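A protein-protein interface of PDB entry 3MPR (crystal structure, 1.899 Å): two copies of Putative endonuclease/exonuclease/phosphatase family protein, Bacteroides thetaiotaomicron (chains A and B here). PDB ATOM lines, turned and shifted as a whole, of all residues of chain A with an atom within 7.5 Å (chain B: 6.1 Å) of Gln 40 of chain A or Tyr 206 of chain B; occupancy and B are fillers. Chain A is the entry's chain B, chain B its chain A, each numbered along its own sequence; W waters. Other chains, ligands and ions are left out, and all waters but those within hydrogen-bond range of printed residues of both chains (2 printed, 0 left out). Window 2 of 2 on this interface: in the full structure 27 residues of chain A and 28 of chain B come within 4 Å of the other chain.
The side-chain amide nitrogen (NE2) of Gln 37 of chain A sits at hydrogen-bond distance from the backbone carbonyl oxygen (O) of Arg 207 of chain B (2.9 Å). NH1 of Arg 240 of chain B is in hydrogen-bond range of O of Gln 40 of chain A (3.2 Å). The side-chain amide oxygen of Gln 40 of chain A is in hydrogen-bond range of the side-chain hydroxyl of Tyr 206 of chain B (2.6 Å). NE2 of Gln 37 of chain A sits at hydrogen-bond distance from OH of Tyr 206 of chain B (3.2 Å). NH2 of Arg 240 of chain B lies within salt-bridge range of OD2 of Asp 43 of chain A, at 2.9 Å. NH1 of Arg 240 of chain B is in hydrogen-bond range of O of Tyr 41 of chain A, at 3.2 Å.
O of Tyr 241 of chain B is in hydrogen-bond range of N of Tyr 208 of chain B, 2.8 Å away. The side-chain sulfur of Cys 204 of chain B sits at hydrogen-bond distance from the backbone carbonyl oxygen of Tyr 206 of chain B. The backbone carbonyl oxygen of Lys 239 of chain B lies within hydrogen-bond range of the backbone NH of Tyr 206 of chain B (3.0 Å). The backbone carbonyl oxygen (O) of Met 38 of chain A sits close to a ring nitrogen (ND1) of His 42 of chain A (3.3 Å). O of Tyr 206 of chain B lies within hydrogen-bond range of N of Tyr 241 of chain B (2.9 Å).
CE1 of Tyr 208 of chain B touches CB of Gln 37 of chain A (3.9 Å). CG of Met 38 of chain A touches OH of Tyr 208 of chain B (3.4 Å). Tyr 41 of chain A touches Tyr 208 of chain B (CG to CD2, 3.3 Å). Tyr 241 of chain B touches Tyr 41 of chain A. CA of Gly 242 of chain B touches OH of Tyr 41 of chain A, 3.5 Å away.
Of the printed residues of chain B, Gln 37 of chain A touches Tyr 206, Arg 207 and Tyr 208. Tyr 206 of chain B touches two residues of chain A. Val 238 of chain B touches none of the printed residues of chain A. Printed residues of chain A within 4 Å of Arg 240 of chain B: Gln 40 (3.2 Å), Tyr 41 (3.2 Å) and Asp 43 (2.9 Å). Printed residues of chain A within 4 Å of Tyr 241 of chain B: Tyr 41 (3.9 Å). The nearest residue of chain A that does not touch Tyr 206 of chain B is Tyr 41 of chain A (4.3 Å). The nearest printed residue of chain B that does not touch Gln 37 of chain A is Arg 240 of chain B (6.9 Å).
Of the 10 printed residues of chain B, 6 touch a printed residue of chain A. Hydrophobic or aromatic side chains of chain B within 4 Å of the printed part of chain A: Tyr 206 and Tyr 208. Printed residues of chain A that touch a printed residue of chain B: Gln 37, Met 38, Gln 40, Tyr 41 and Asp 43. Hydrophobic or aromatic side chains of chain A within 4 Å of the printed part of chain B: Met 38 and Tyr 41. Among the printed residues, 11 pairs touch across the chains.
No position is printed for both chains. Of the 11 pairs that touch across the chains among the printed residues, none has its exchanged pair printed and touching as well.
Water W2 lies within hydrogen-bond range of the side-chain hydroxyl (OH) of Tyr 41 of chain A (2.7 Å), the backbone carbonyl oxygen (O) of Arg 240 of chain B (3.4 Å) and the backbone NH (N) of Gly 242 of chain B (3.4 Å). Water W1 lies within hydrogen-bond range of NH1 of Arg 240 of chain B (3.0 Å) and O of Gln 40 of chain A (3.1 Å).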
ATOM      1  N   PRO A  33      29.106  -8.257 -22.627  1.00  0.00           N
ATOM      2  CA  PRO A  33      29.519  -9.401 -21.808  1.00  0.00           C
ATOM      3  C   PRO A  33      29.890  -8.951 -20.402  1.00  0.00           C
ATOM      4  O   PRO A  33      29.690  -9.706 -19.454  1.00  0.00           O
ATOM      5  CB  PRO A  33      30.748  -9.940 -22.555  1.00  0.00           C
ATOM      6  CG  PRO A  33      30.477  -9.554 -23.989  1.00  0.00           C
ATOM      7  CD  PRO A  33      29.886  -8.179 -23.878  1.00  0.00           C
ATOM      8  N   VAL A  34      30.412  -7.735 -20.271  1.00  0.00           N
ATOM      9  CA  VAL A  34      30.794  -7.217 -18.958  1.00  0.00           C
ATOM     10  C   VAL A  34      29.562  -6.814 -18.151  1.00  0.00           C
ATOM     11  O   VAL A  34      29.461  -7.116 -16.966  1.00  0.00           O
ATOM     12  CB  VAL A  34      31.794  -6.045 -19.073  1.00  0.00           C
ATOM     13  CG1 VAL A  34      32.146  -5.485 -17.682  1.00  0.00           C
ATOM     14  CG2 VAL A  34      33.069  -6.525 -19.774  1.00  0.00           C
ATOM     15  N   ILE A  35      28.627  -6.139 -18.809  1.00  0.00           N
ATOM     16  CA  ILE A  35      27.339  -5.800 -18.216  1.00  0.00           C
ATOM     17  C   ILE A  35      26.644  -7.051 -17.675  1.00  0.00           C
ATOM     18  O   ILE A  35      26.152  -7.064 -16.553  1.00  0.00           O
ATOM     19  CB  ILE A  35      26.406  -5.148 -19.262  1.00  0.00           C
ATOM     20  CG1 ILE A  35      26.946  -3.766 -19.678  1.00  0.00           C
ATOM     21  CG2 ILE A  35      24.955  -5.082 -18.719  1.00  0.00           C
ATOM     22  CD1 ILE A  35      26.153  -3.096 -20.823  1.00  0.00           C
ATOM     23  N   ALA A  36      26.601  -8.104 -18.486  1.00  0.00           N
ATOM     24  CA  ALA A  36      25.984  -9.358 -18.061  1.00  0.00           C
ATOM     25  C   ALA A  36      26.672  -9.943 -16.828  1.00  0.00           C
ATOM     26  O   ALA A  36      26.013 -10.470 -15.928  1.00  0.00           O
ATOM     27  CB  ALA A  36      25.988 -10.383 -19.199  1.00  0.00           C
ATOM     28  N   GLN A  37      27.995  -9.886 -16.801  1.00  0.00           N
ATOM     29  CA  GLN A  37      28.718 -10.352 -15.622  1.00  0.00           C
ATOM     30  C   GLN A  37      28.363  -9.533 -14.374  1.00  0.00           C
ATOM     31  O   GLN A  37      28.213 -10.085 -13.288  1.00  0.00           O
ATOM     32  CB  GLN A  37      30.226 -10.343 -15.859  1.00  0.00           C
ATOM     33  CG  GLN A  37      30.752 -11.538 -16.660  1.00  0.00           C
ATOM     34  CD  GLN A  37      32.080 -12.044 -16.112  1.00  0.00           C
ATOM     35  OE1 GLN A  37      33.137 -11.524 -16.448  1.00  0.00           O
ATOM     36  NE2 GLN A  37      32.021 -13.048 -15.238  1.00  0.00           N
ATOM     37  N   MET A  38      28.207  -8.222 -14.529  1.00  0.00           N
ATOM     38  CA  MET A  38      27.811  -7.391 -13.400  1.00  0.00           C
ATOM     39  C   MET A  38      26.438  -7.758 -12.874  1.00  0.00           C
ATOM     40  O   MET A  38      26.216  -7.813 -11.664  1.00  0.00           O
ATOM     41  CB  MET A  38      27.829  -5.905 -13.785  1.00  0.00           C
ATOM     42  CG  MET A  38      29.230  -5.366 -13.953  1.00  0.00           C
ATOM     43  SD  MET A  38      29.142  -3.459 -14.336  1.00  0.00           S
ATOM     44  CE  MET A  38      28.660  -2.845 -12.540  1.00  0.00           C
ATOM     45  N   VAL A  39      25.500  -7.963 -13.789  1.00  0.00           N
ATOM     46  CA  VAL A  39      24.168  -8.420 -13.421  1.00  0.00           C
ATOM     47  C   VAL A  39      24.242  -9.681 -12.554  1.00  0.00           C
ATOM     48  O   VAL A  39      23.578  -9.791 -11.512  1.00  0.00           O
ATOM     49  CB  VAL A  39      23.328  -8.723 -14.687  1.00  0.00           C
ATOM     50  CG1 VAL A  39      22.045  -9.468 -14.313  1.00  0.00           C
ATOM     51  CG2 VAL A  39      23.023  -7.424 -15.429  1.00  0.00           C
ATOM     52  N   GLN A  40      25.072 -10.627 -12.974  1.00  0.00           N
ATOM     53  CA  GLN A  40      25.166 -11.901 -12.263  1.00  0.00           C
ATOM     54  C   GLN A  40      25.943 -11.749 -10.950  1.00  0.00           C
ATOM     55  O   GLN A  40      25.510 -12.237  -9.915  1.00  0.00           O
ATOM     56  CB  GLN A  40      25.845 -12.960 -13.148  1.00  0.00           C
ATOM     57  CG  GLN A  40      25.030 -13.370 -14.399  1.00  0.00           C
ATOM     58  CD  GLN A  40      25.841 -14.188 -15.394  1.00  0.00           C
ATOM     59  OE1 GLN A  40      27.020 -13.911 -15.638  1.00  0.00           O
ATOM     60  NE2 GLN A  40      25.205 -15.201 -15.982  1.00  0.00           N
ATOM     61  N   TYR A  41      27.093 -11.083 -11.002  1.00  0.00           N
ATOM     62  CA  TYR A  41      27.957 -10.980  -9.818  1.00  0.00           C
ATOM     63  C   TYR A  41      27.292 -10.164  -8.717  1.00  0.00           C
ATOM     64  O   TYR A  41      27.450 -10.437  -7.511  1.00  0.00           O
ATOM     65  CB  TYR A  41      29.293 -10.312 -10.164  1.00  0.00           C
ATOM     66  CG  TYR A  41      30.231 -10.339  -8.980  1.00  0.00           C
ATOM     67  CD1 TYR A  41      30.862 -11.512  -8.621  1.00  0.00           C
ATOM     68  CD2 TYR A  41      30.431  -9.213  -8.182  1.00  0.00           C
ATOM     69  CE1 TYR A  41      31.715 -11.570  -7.517  1.00  0.00           C
ATOM     70  CE2 TYR A  41      31.285  -9.260  -7.070  1.00  0.00           C
ATOM     71  CZ  TYR A  41      31.918 -10.450  -6.747  1.00  0.00           C
ATOM     72  OH  TYR A  41      32.760 -10.547  -5.642  1.00  0.00           O
ATOM     73  N   HIS A  42      26.563  -9.139  -9.134  1.00  0.00           N
ATOM     74  CA  HIS A  42      25.933  -8.233  -8.185  1.00  0.00           C
ATOM     75  C   HIS A  42      24.512  -8.662  -7.829  1.00  0.00           C
ATOM     76  O   HIS A  42      23.821  -7.970  -7.098  1.00  0.00           O
ATOM     77  CB  HIS A  42      25.996  -6.793  -8.706  1.00  0.00           C
ATOM     78  CG  HIS A  42      27.370  -6.209  -8.635  1.00  0.00           C
ATOM     79  ND1 HIS A  42      28.163  -6.020  -9.748  1.00  0.00           N
ATOM     80  CD2 HIS A  42      28.105  -5.796  -7.575  1.00  0.00           C
ATOM     81  CE1 HIS A  42      29.320  -5.499  -9.378  1.00  0.00           C
ATOM     82  NE2 HIS A  42      29.314  -5.361  -8.065  1.00  0.00           N
ATOM     83  N   ASP A  43      24.091  -9.818  -8.339  1.00  0.00           N
ATOM     84  CA  ASP A  43      22.869 -10.473  -7.860  1.00  0.00           C
ATOM     85  C   ASP A  43      21.577  -9.692  -8.096  1.00  0.00           C
ATOM     86  O   ASP A  43      20.706  -9.659  -7.221  1.00  0.00           O
ATOM     87  CB  ASP A  43      22.982 -10.794  -6.360  1.00  0.00           C
ATOM     88  CG  ASP A  43      24.026 -11.849  -6.069  1.00  0.00           C
ATOM     89  OD1 ASP A  43      24.216 -12.734  -6.916  1.00  0.00           O
ATOM     90  OD2 ASP A  43      24.669 -11.780  -5.004  1.00  0.00           O
ATOM     91  N   PHE A  44      21.433  -9.090  -9.272  1.00  0.00           N
ATOM     92  CA  PHE A  44      20.193  -8.394  -9.608  1.00  0.00           C
ATOM     93  C   PHE A  44      19.066  -9.417  -9.740  1.00  0.00           C
ATOM     94  O   PHE A  44      19.124 -10.284 -10.611  1.00  0.00           O
ATOM     95  CB  PHE A  44      20.323  -7.674 -10.955  1.00  0.00           C
ATOM     96  CG  PHE A  44      21.325  -6.541 -10.973  1.00  0.00           C
ATOM     97  CD1 PHE A  44      22.062  -6.204  -9.845  1.00  0.00           C
ATOM     98  CD2 PHE A  44      21.521  -5.811 -12.146  1.00  0.00           C
ATOM     99  CE1 PHE A  44      22.981  -5.162  -9.886  1.00  0.00           C
ATOM    100  CE2 PHE A  44      22.424  -4.767 -12.198  1.00  0.00           C
ATOM    101  CZ  PHE A  44      23.170  -4.442 -11.065  1.00  0.00           C
ATOM    102  N   PHE A  47      15.622  -6.039 -12.794  1.00  0.00           N
ATOM    103  CA  PHE A  47      16.191  -4.733 -13.074  1.00  0.00           C
ATOM    104  C   PHE A  47      15.609  -4.088 -14.319  1.00  0.00           C
ATOM    105  O   PHE A  47      15.295  -4.774 -15.285  1.00  0.00           O
ATOM    106  CB  PHE A  47      17.724  -4.787 -13.159  1.00  0.00           C
ATOM    107  CG  PHE A  47      18.269  -5.677 -14.260  1.00  0.00           C
ATOM    108  CD1 PHE A  47      18.317  -7.055 -14.099  1.00  0.00           C
ATOM    109  CD2 PHE A  47      18.781  -5.130 -15.427  1.00  0.00           C
ATOM    110  CE1 PHE A  47      18.840  -7.869 -15.091  1.00  0.00           C
ATOM    111  CE2 PHE A  47      19.305  -5.930 -16.434  1.00  0.00           C
ATOM    112  CZ  PHE A  47      19.335  -7.314 -16.268  1.00  0.00           C
ATOM    113  N   GLU A  62      20.819 -14.078 -24.028  1.00  0.00           N
ATOM    114  CA  GLU A  62      21.757 -15.176 -24.278  1.00  0.00           C
ATOM    115  C   GLU A  62      22.852 -15.233 -23.212  1.00  0.00           C
ATOM    116  O   GLU A  62      23.274 -16.316 -22.793  1.00  0.00           O
ATOM    117  CB  GLU A  62      22.387 -15.029 -25.663  1.00  0.00           C
ATOM    118  CG  GLU A  62      23.357 -16.141 -26.027  1.00  0.00           C
ATOM    119  CD  GLU A  62      23.898 -16.000 -27.442  1.00  0.00           C
ATOM    120  OE1 GLU A  62      23.910 -14.862 -27.965  1.00  0.00           O
ATOM    121  OE2 GLU A  62      24.306 -17.027 -28.031  1.00  0.00           O
ATOM    122  N   ALA A  63      23.316 -14.066 -22.778  1.00  0.00           N
ATOM    123  CA  ALA A  63      24.359 -13.998 -21.761  1.00  0.00           C
ATOM    124  C   ALA A  63      23.805 -14.207 -20.341  1.00  0.00           C
ATOM    125  O   ALA A  63      24.571 -14.351 -19.380  1.00  0.00           O
ATOM    126  CB  ALA A  63      25.088 -12.654 -21.853  1.00  0.00           C
ATOM    127  N   LEU A  64      22.480 -14.202 -20.206  1.00  0.00           N
ATOM    128  CA  LEU A  64      21.842 -14.290 -18.889  1.00  0.00           C
ATOM    129  C   LEU A  64      20.800 -15.406 -18.887  1.00  0.00           C
ATOM    130  O   LEU A  64      19.599 -15.150 -18.803  1.00  0.00           O
ATOM    131  CB  LEU A  64      21.184 -12.958 -18.527  1.00  0.00           C
ATOM    132  CG  LEU A  64      22.065 -11.720 -18.269  1.00  0.00           C
ATOM    133  CD1 LEU A  64      21.152 -10.520 -18.105  1.00  0.00           C
ATOM    134  CD2 LEU A  64      22.993 -11.865 -17.039  1.00  0.00           C
ATOM    135  N   PRO A  65      21.260 -16.661 -18.973  1.00  0.00           N
ATOM    136  CA  PRO A  65      20.330 -17.766 -19.229  1.00  0.00           C
ATOM    137  C   PRO A  65      19.224 -17.943 -18.178  1.00  0.00           C
ATOM    138  O   PRO A  65      18.178 -18.508 -18.503  1.00  0.00           O
ATOM    139  CB  PRO A  65      21.250 -18.995 -19.287  1.00  0.00           C
ATOM    140  CG  PRO A  65      22.470 -18.597 -18.536  1.00  0.00           C
ATOM    141  CD  PRO A  65      22.649 -17.127 -18.827  1.00  0.00           C
ATOM    142  N   GLY A  66      19.431 -17.474 -16.953  1.00  0.00           N
ATOM    143  CA  GLY A  66      18.379 -17.584 -15.949  1.00  0.00           C
ATOM    144  C   GLY A  66      17.388 -16.423 -15.934  1.00  0.00           C
ATOM    145  O   GLY A  66      16.558 -16.314 -15.021  1.00  0.00           O
ATOM    146  N   TYR A  67      17.462 -15.565 -16.949  1.00  0.00           N
ATOM    147  CA  TYR A  67      16.639 -14.355 -16.994  1.00  0.00           C
ATOM    148  C   TYR A  67      15.746 -14.317 -18.236  1.00  0.00           C
ATOM    149  O   TYR A  67      16.061 -14.894 -19.270  1.00  0.00           O
ATOM    150  CB  TYR A  67      17.533 -13.098 -17.011  1.00  0.00           C
ATOM    151  CG  TYR A  67      18.269 -12.794 -15.719  1.00  0.00           C
ATOM    152  CD1 TYR A  67      17.858 -11.748 -14.888  1.00  0.00           C
ATOM    153  CD2 TYR A  67      19.389 -13.524 -15.342  1.00  0.00           C
ATOM    154  CE1 TYR A  67      18.548 -11.443 -13.704  1.00  0.00           C
ATOM    155  CE2 TYR A  67      20.078 -13.228 -14.164  1.00  0.00           C
ATOM    156  CZ  TYR A  67      19.650 -12.189 -13.353  1.00  0.00           C
ATOM    157  OH  TYR A  67      20.344 -11.906 -12.193  1.00  0.00           O
ATOM    158  N   ARG A  89      14.775 -12.690 -12.927  1.00  0.00           N
ATOM    159  CA  ARG A  89      15.133 -14.093 -12.749  1.00  0.00           C
ATOM    160  C   ARG A  89      13.899 -14.973 -12.824  1.00  0.00           C
ATOM    161  O   ARG A  89      12.979 -14.837 -12.007  1.00  0.00           O
ATOM    162  CB  ARG A  89      15.793 -14.315 -11.380  1.00  0.00           C
ATOM    163  CG  ARG A  89      17.203 -13.809 -11.292  1.00  0.00           C
ATOM    164  CD  ARG A  89      17.857 -14.197  -9.958  1.00  0.00           C
ATOM    165  NE  ARG A  89      17.870 -15.652  -9.778  1.00  0.00           N
ATOM    166  CZ  ARG A  89      18.675 -16.285  -8.935  1.00  0.00           C
ATOM    167  NH1 ARG A  89      19.535 -15.587  -8.194  1.00  0.00           N
ATOM    168  NH2 ARG A  89      18.627 -17.614  -8.835  1.00  0.00           N
ATOM    169  N   CYS B 204      36.410 -21.762  -8.121  1.00  0.00           N
ATOM    170  CA  CYS B 204      35.101 -21.133  -8.005  1.00  0.00           C
ATOM    171  C   CYS B 204      34.127 -21.659  -9.071  1.00  0.00           C
ATOM    172  O   CYS B 204      34.537 -21.973 -10.181  1.00  0.00           O
ATOM    173  CB  CYS B 204      35.224 -19.602  -8.136  1.00  0.00           C
ATOM    174  SG  CYS B 204      35.910 -19.030  -9.710  1.00  0.00           S
ATOM    175  N   ASP B 205      32.845 -21.752  -8.721  1.00  0.00           N
ATOM    176  CA  ASP B 205      31.793 -21.961  -9.721  1.00  0.00           C
ATOM    177  C   ASP B 205      31.677 -20.766 -10.651  1.00  0.00           C
ATOM    178  O   ASP B 205      31.567 -20.924 -11.872  1.00  0.00           O
ATOM    179  CB  ASP B 205      30.436 -22.179  -9.053  1.00  0.00           C
ATOM    180  CG  ASP B 205      30.382 -23.460  -8.237  1.00  0.00           C
ATOM    181  OD1 ASP B 205      31.108 -24.412  -8.573  1.00  0.00           O
ATOM    182  OD2 ASP B 205      29.610 -23.503  -7.259  1.00  0.00           O
ATOM    183  N   TYR B 206      31.683 -19.575 -10.059  1.00  0.00           N
ATOM    184  CA  TYR B 206      31.498 -18.334 -10.798  1.00  0.00           C
ATOM    185  C   TYR B 206      32.700 -17.389 -10.631  1.00  0.00           C
ATOM    186  O   TYR B 206      33.057 -17.015  -9.513  1.00  0.00           O
ATOM    187  CB  TYR B 206      30.187 -17.635 -10.398  1.00  0.00           C
ATOM    188  CG  TYR B 206      29.855 -16.506 -11.351  1.00  0.00           C
ATOM    189  CD1 TYR B 206      28.993 -16.707 -12.423  1.00  0.00           C
ATOM    190  CD2 TYR B 206      30.458 -15.253 -11.213  1.00  0.00           C
ATOM    191  CE1 TYR B 206      28.722 -15.679 -13.335  1.00  0.00           C
ATOM    192  CE2 TYR B 206      30.191 -14.223 -12.107  1.00  0.00           C
ATOM    193  CZ  TYR B 206      29.327 -14.438 -13.161  1.00  0.00           C
ATOM    194  OH  TYR B 206      29.080 -13.425 -14.058  1.00  0.00           O
ATOM    195  N   ARG B 207      33.317 -17.014 -11.749  1.00  0.00           N
ATOM    196  CA  ARG B 207      34.483 -16.138 -11.729  1.00  0.00           C
ATOM    197  C   ARG B 207      34.177 -14.767 -12.335  1.00  0.00           C
ATOM    198  O   ARG B 207      33.727 -14.667 -13.483  1.00  0.00           O
ATOM    199  CB  ARG B 207      35.652 -16.796 -12.470  1.00  0.00           C
ATOM    200  CG  ARG B 207      36.956 -15.972 -12.481  1.00  0.00           C
ATOM    201  CD  ARG B 207      37.970 -16.569 -13.453  1.00  0.00           C
ATOM    202  NE  ARG B 207      38.438 -17.884 -13.031  1.00  0.00           N
ATOM    203  CZ  ARG B 207      38.873 -18.832 -13.856  1.00  0.00           C
ATOM    204  NH1 ARG B 207      38.893 -18.632 -15.170  1.00  0.00           N
ATOM    205  NH2 ARG B 207      39.278 -19.995 -13.363  1.00  0.00           N
ATOM    206  N   TYR B 208      34.416 -13.723 -11.543  1.00  0.00           N
ATOM    207  CA  TYR B 208      34.264 -12.331 -11.961  1.00  0.00           C
ATOM    208  C   TYR B 208      35.630 -11.664 -11.819  1.00  0.00           C
ATOM    209  O   TYR B 208      36.029 -11.272 -10.729  1.00  0.00           O
ATOM    210  CB  TYR B 208      33.227 -11.624 -11.072  1.00  0.00           C
ATOM    211  CG  TYR B 208      32.946 -10.187 -11.452  1.00  0.00           C
ATOM    212  CD1 TYR B 208      32.663  -9.840 -12.760  1.00  0.00           C
ATOM    213  CD2 TYR B 208      32.961  -9.180 -10.494  1.00  0.00           C
ATOM    214  CE1 TYR B 208      32.412  -8.529 -13.116  1.00  0.00           C
ATOM    215  CE2 TYR B 208      32.699  -7.863 -10.838  1.00  0.00           C
ATOM    216  CZ  TYR B 208      32.421  -7.553 -12.153  1.00  0.00           C
ATOM    217  OH  TYR B 208      32.155  -6.259 -12.506  1.00  0.00           O
ATOM    218  N   VAL B 238      33.834 -23.574  -3.267  1.00  0.00           N
ATOM    219  CA  VAL B 238      34.066 -22.179  -3.619  1.00  0.00           C
ATOM    220  C   VAL B 238      32.971 -21.763  -4.608  1.00  0.00           C
ATOM    221  O   VAL B 238      32.962 -22.210  -5.752  1.00  0.00           O
ATOM    222  CB  VAL B 238      35.464 -21.959  -4.237  1.00  0.00           C
ATOM    223  CG1 VAL B 238      35.667 -20.482  -4.574  1.00  0.00           C
ATOM    224  CG2 VAL B 238      36.570 -22.436  -3.269  1.00  0.00           C
ATOM    225  N   LYS B 239      32.045 -20.933  -4.144  1.00  0.00           N
ATOM    226  CA  LYS B 239      30.906 -20.518  -4.950  1.00  0.00           C
ATOM    227  C   LYS B 239      31.301 -19.434  -5.952  1.00  0.00           C
ATOM    228  O   LYS B 239      30.945 -19.503  -7.132  1.00  0.00           O
ATOM    229  CB  LYS B 239      29.782 -19.997  -4.053  1.00  0.00           C
ATOM    230  CG  LYS B 239      29.305 -20.992  -3.000  1.00  0.00           C
ATOM    231  CD  LYS B 239      28.314 -21.998  -3.576  1.00  0.00           C
ATOM    232  CE  LYS B 239      27.001 -21.317  -3.962  1.00  0.00           C
ATOM    233  NZ  LYS B 239      26.009 -22.292  -4.476  1.00  0.00           N
ATOM    234  N   ARG B 240      32.046 -18.432  -5.498  1.00  0.00           N
ATOM    235  CA  ARG B 240      32.250 -17.267  -6.362  1.00  0.00           C
ATOM    236  C   ARG B 240      33.512 -16.509  -5.999  1.00  0.00           C
ATOM    237  O   ARG B 240      33.879 -16.424  -4.834  1.00  0.00           O
ATOM    238  CB  ARG B 240      31.018 -16.348  -6.304  1.00  0.00           C
ATOM    239  CG  ARG B 240      31.006 -15.193  -7.316  1.00  0.00           C
ATOM    240  CD  ARG B 240      29.564 -14.713  -7.595  1.00  0.00           C
ATOM    241  NE  ARG B 240      28.921 -14.167  -6.398  1.00  0.00           N
ATOM    242  CZ  ARG B 240      27.694 -13.657  -6.362  1.00  0.00           C
ATOM    243  NH1 ARG B 240      26.940 -13.620  -7.466  1.00  0.00           N
ATOM    244  NH2 ARG B 240      27.209 -13.187  -5.212  1.00  0.00           N
ATOM    245  N   TYR B 241      34.173 -15.984  -7.024  1.00  0.00           N
ATOM    246  CA  TYR B 241      35.393 -15.215  -6.875  1.00  0.00           C
ATOM    247  C   TYR B 241      35.155 -13.901  -7.607  1.00  0.00           C
ATOM    248  O   TYR B 241      34.626 -13.886  -8.726  1.00  0.00           O
ATOM    249  CB  TYR B 241      36.556 -15.985  -7.511  1.00  0.00           C
ATOM    250  CG  TYR B 241      37.853 -15.212  -7.723  1.00  0.00           C
ATOM    251  CD1 TYR B 241      37.987 -14.317  -8.789  1.00  0.00           C
ATOM    252  CD2 TYR B 241      38.952 -15.405  -6.886  1.00  0.00           C
ATOM    253  CE1 TYR B 241      39.168 -13.630  -9.007  1.00  0.00           C
ATOM    254  CE2 TYR B 241      40.158 -14.725  -7.100  1.00  0.00           C
ATOM    255  CZ  TYR B 241      40.258 -13.842  -8.158  1.00  0.00           C
ATOM    256  OH  TYR B 241      41.430 -13.151  -8.382  1.00  0.00           O
ATOM    257  N   GLY B 242      35.528 -12.798  -6.975  1.00  0.00           N
ATOM    258  CA  GLY B 242      35.443 -11.503  -7.621  1.00  0.00           C
ATOM    259  C   GLY B 242      36.632 -10.625  -7.279  1.00  0.00           C
ATOM    260  O   GLY B 242      37.135 -10.645  -6.161  1.00  0.00           O
HETATM  261  O   HOH W   1      27.284 -14.744 -10.172  1.00  0.00           O
HETATM  262  O   HOH W   2      32.834 -13.159  -4.858  1.00  0.00           O
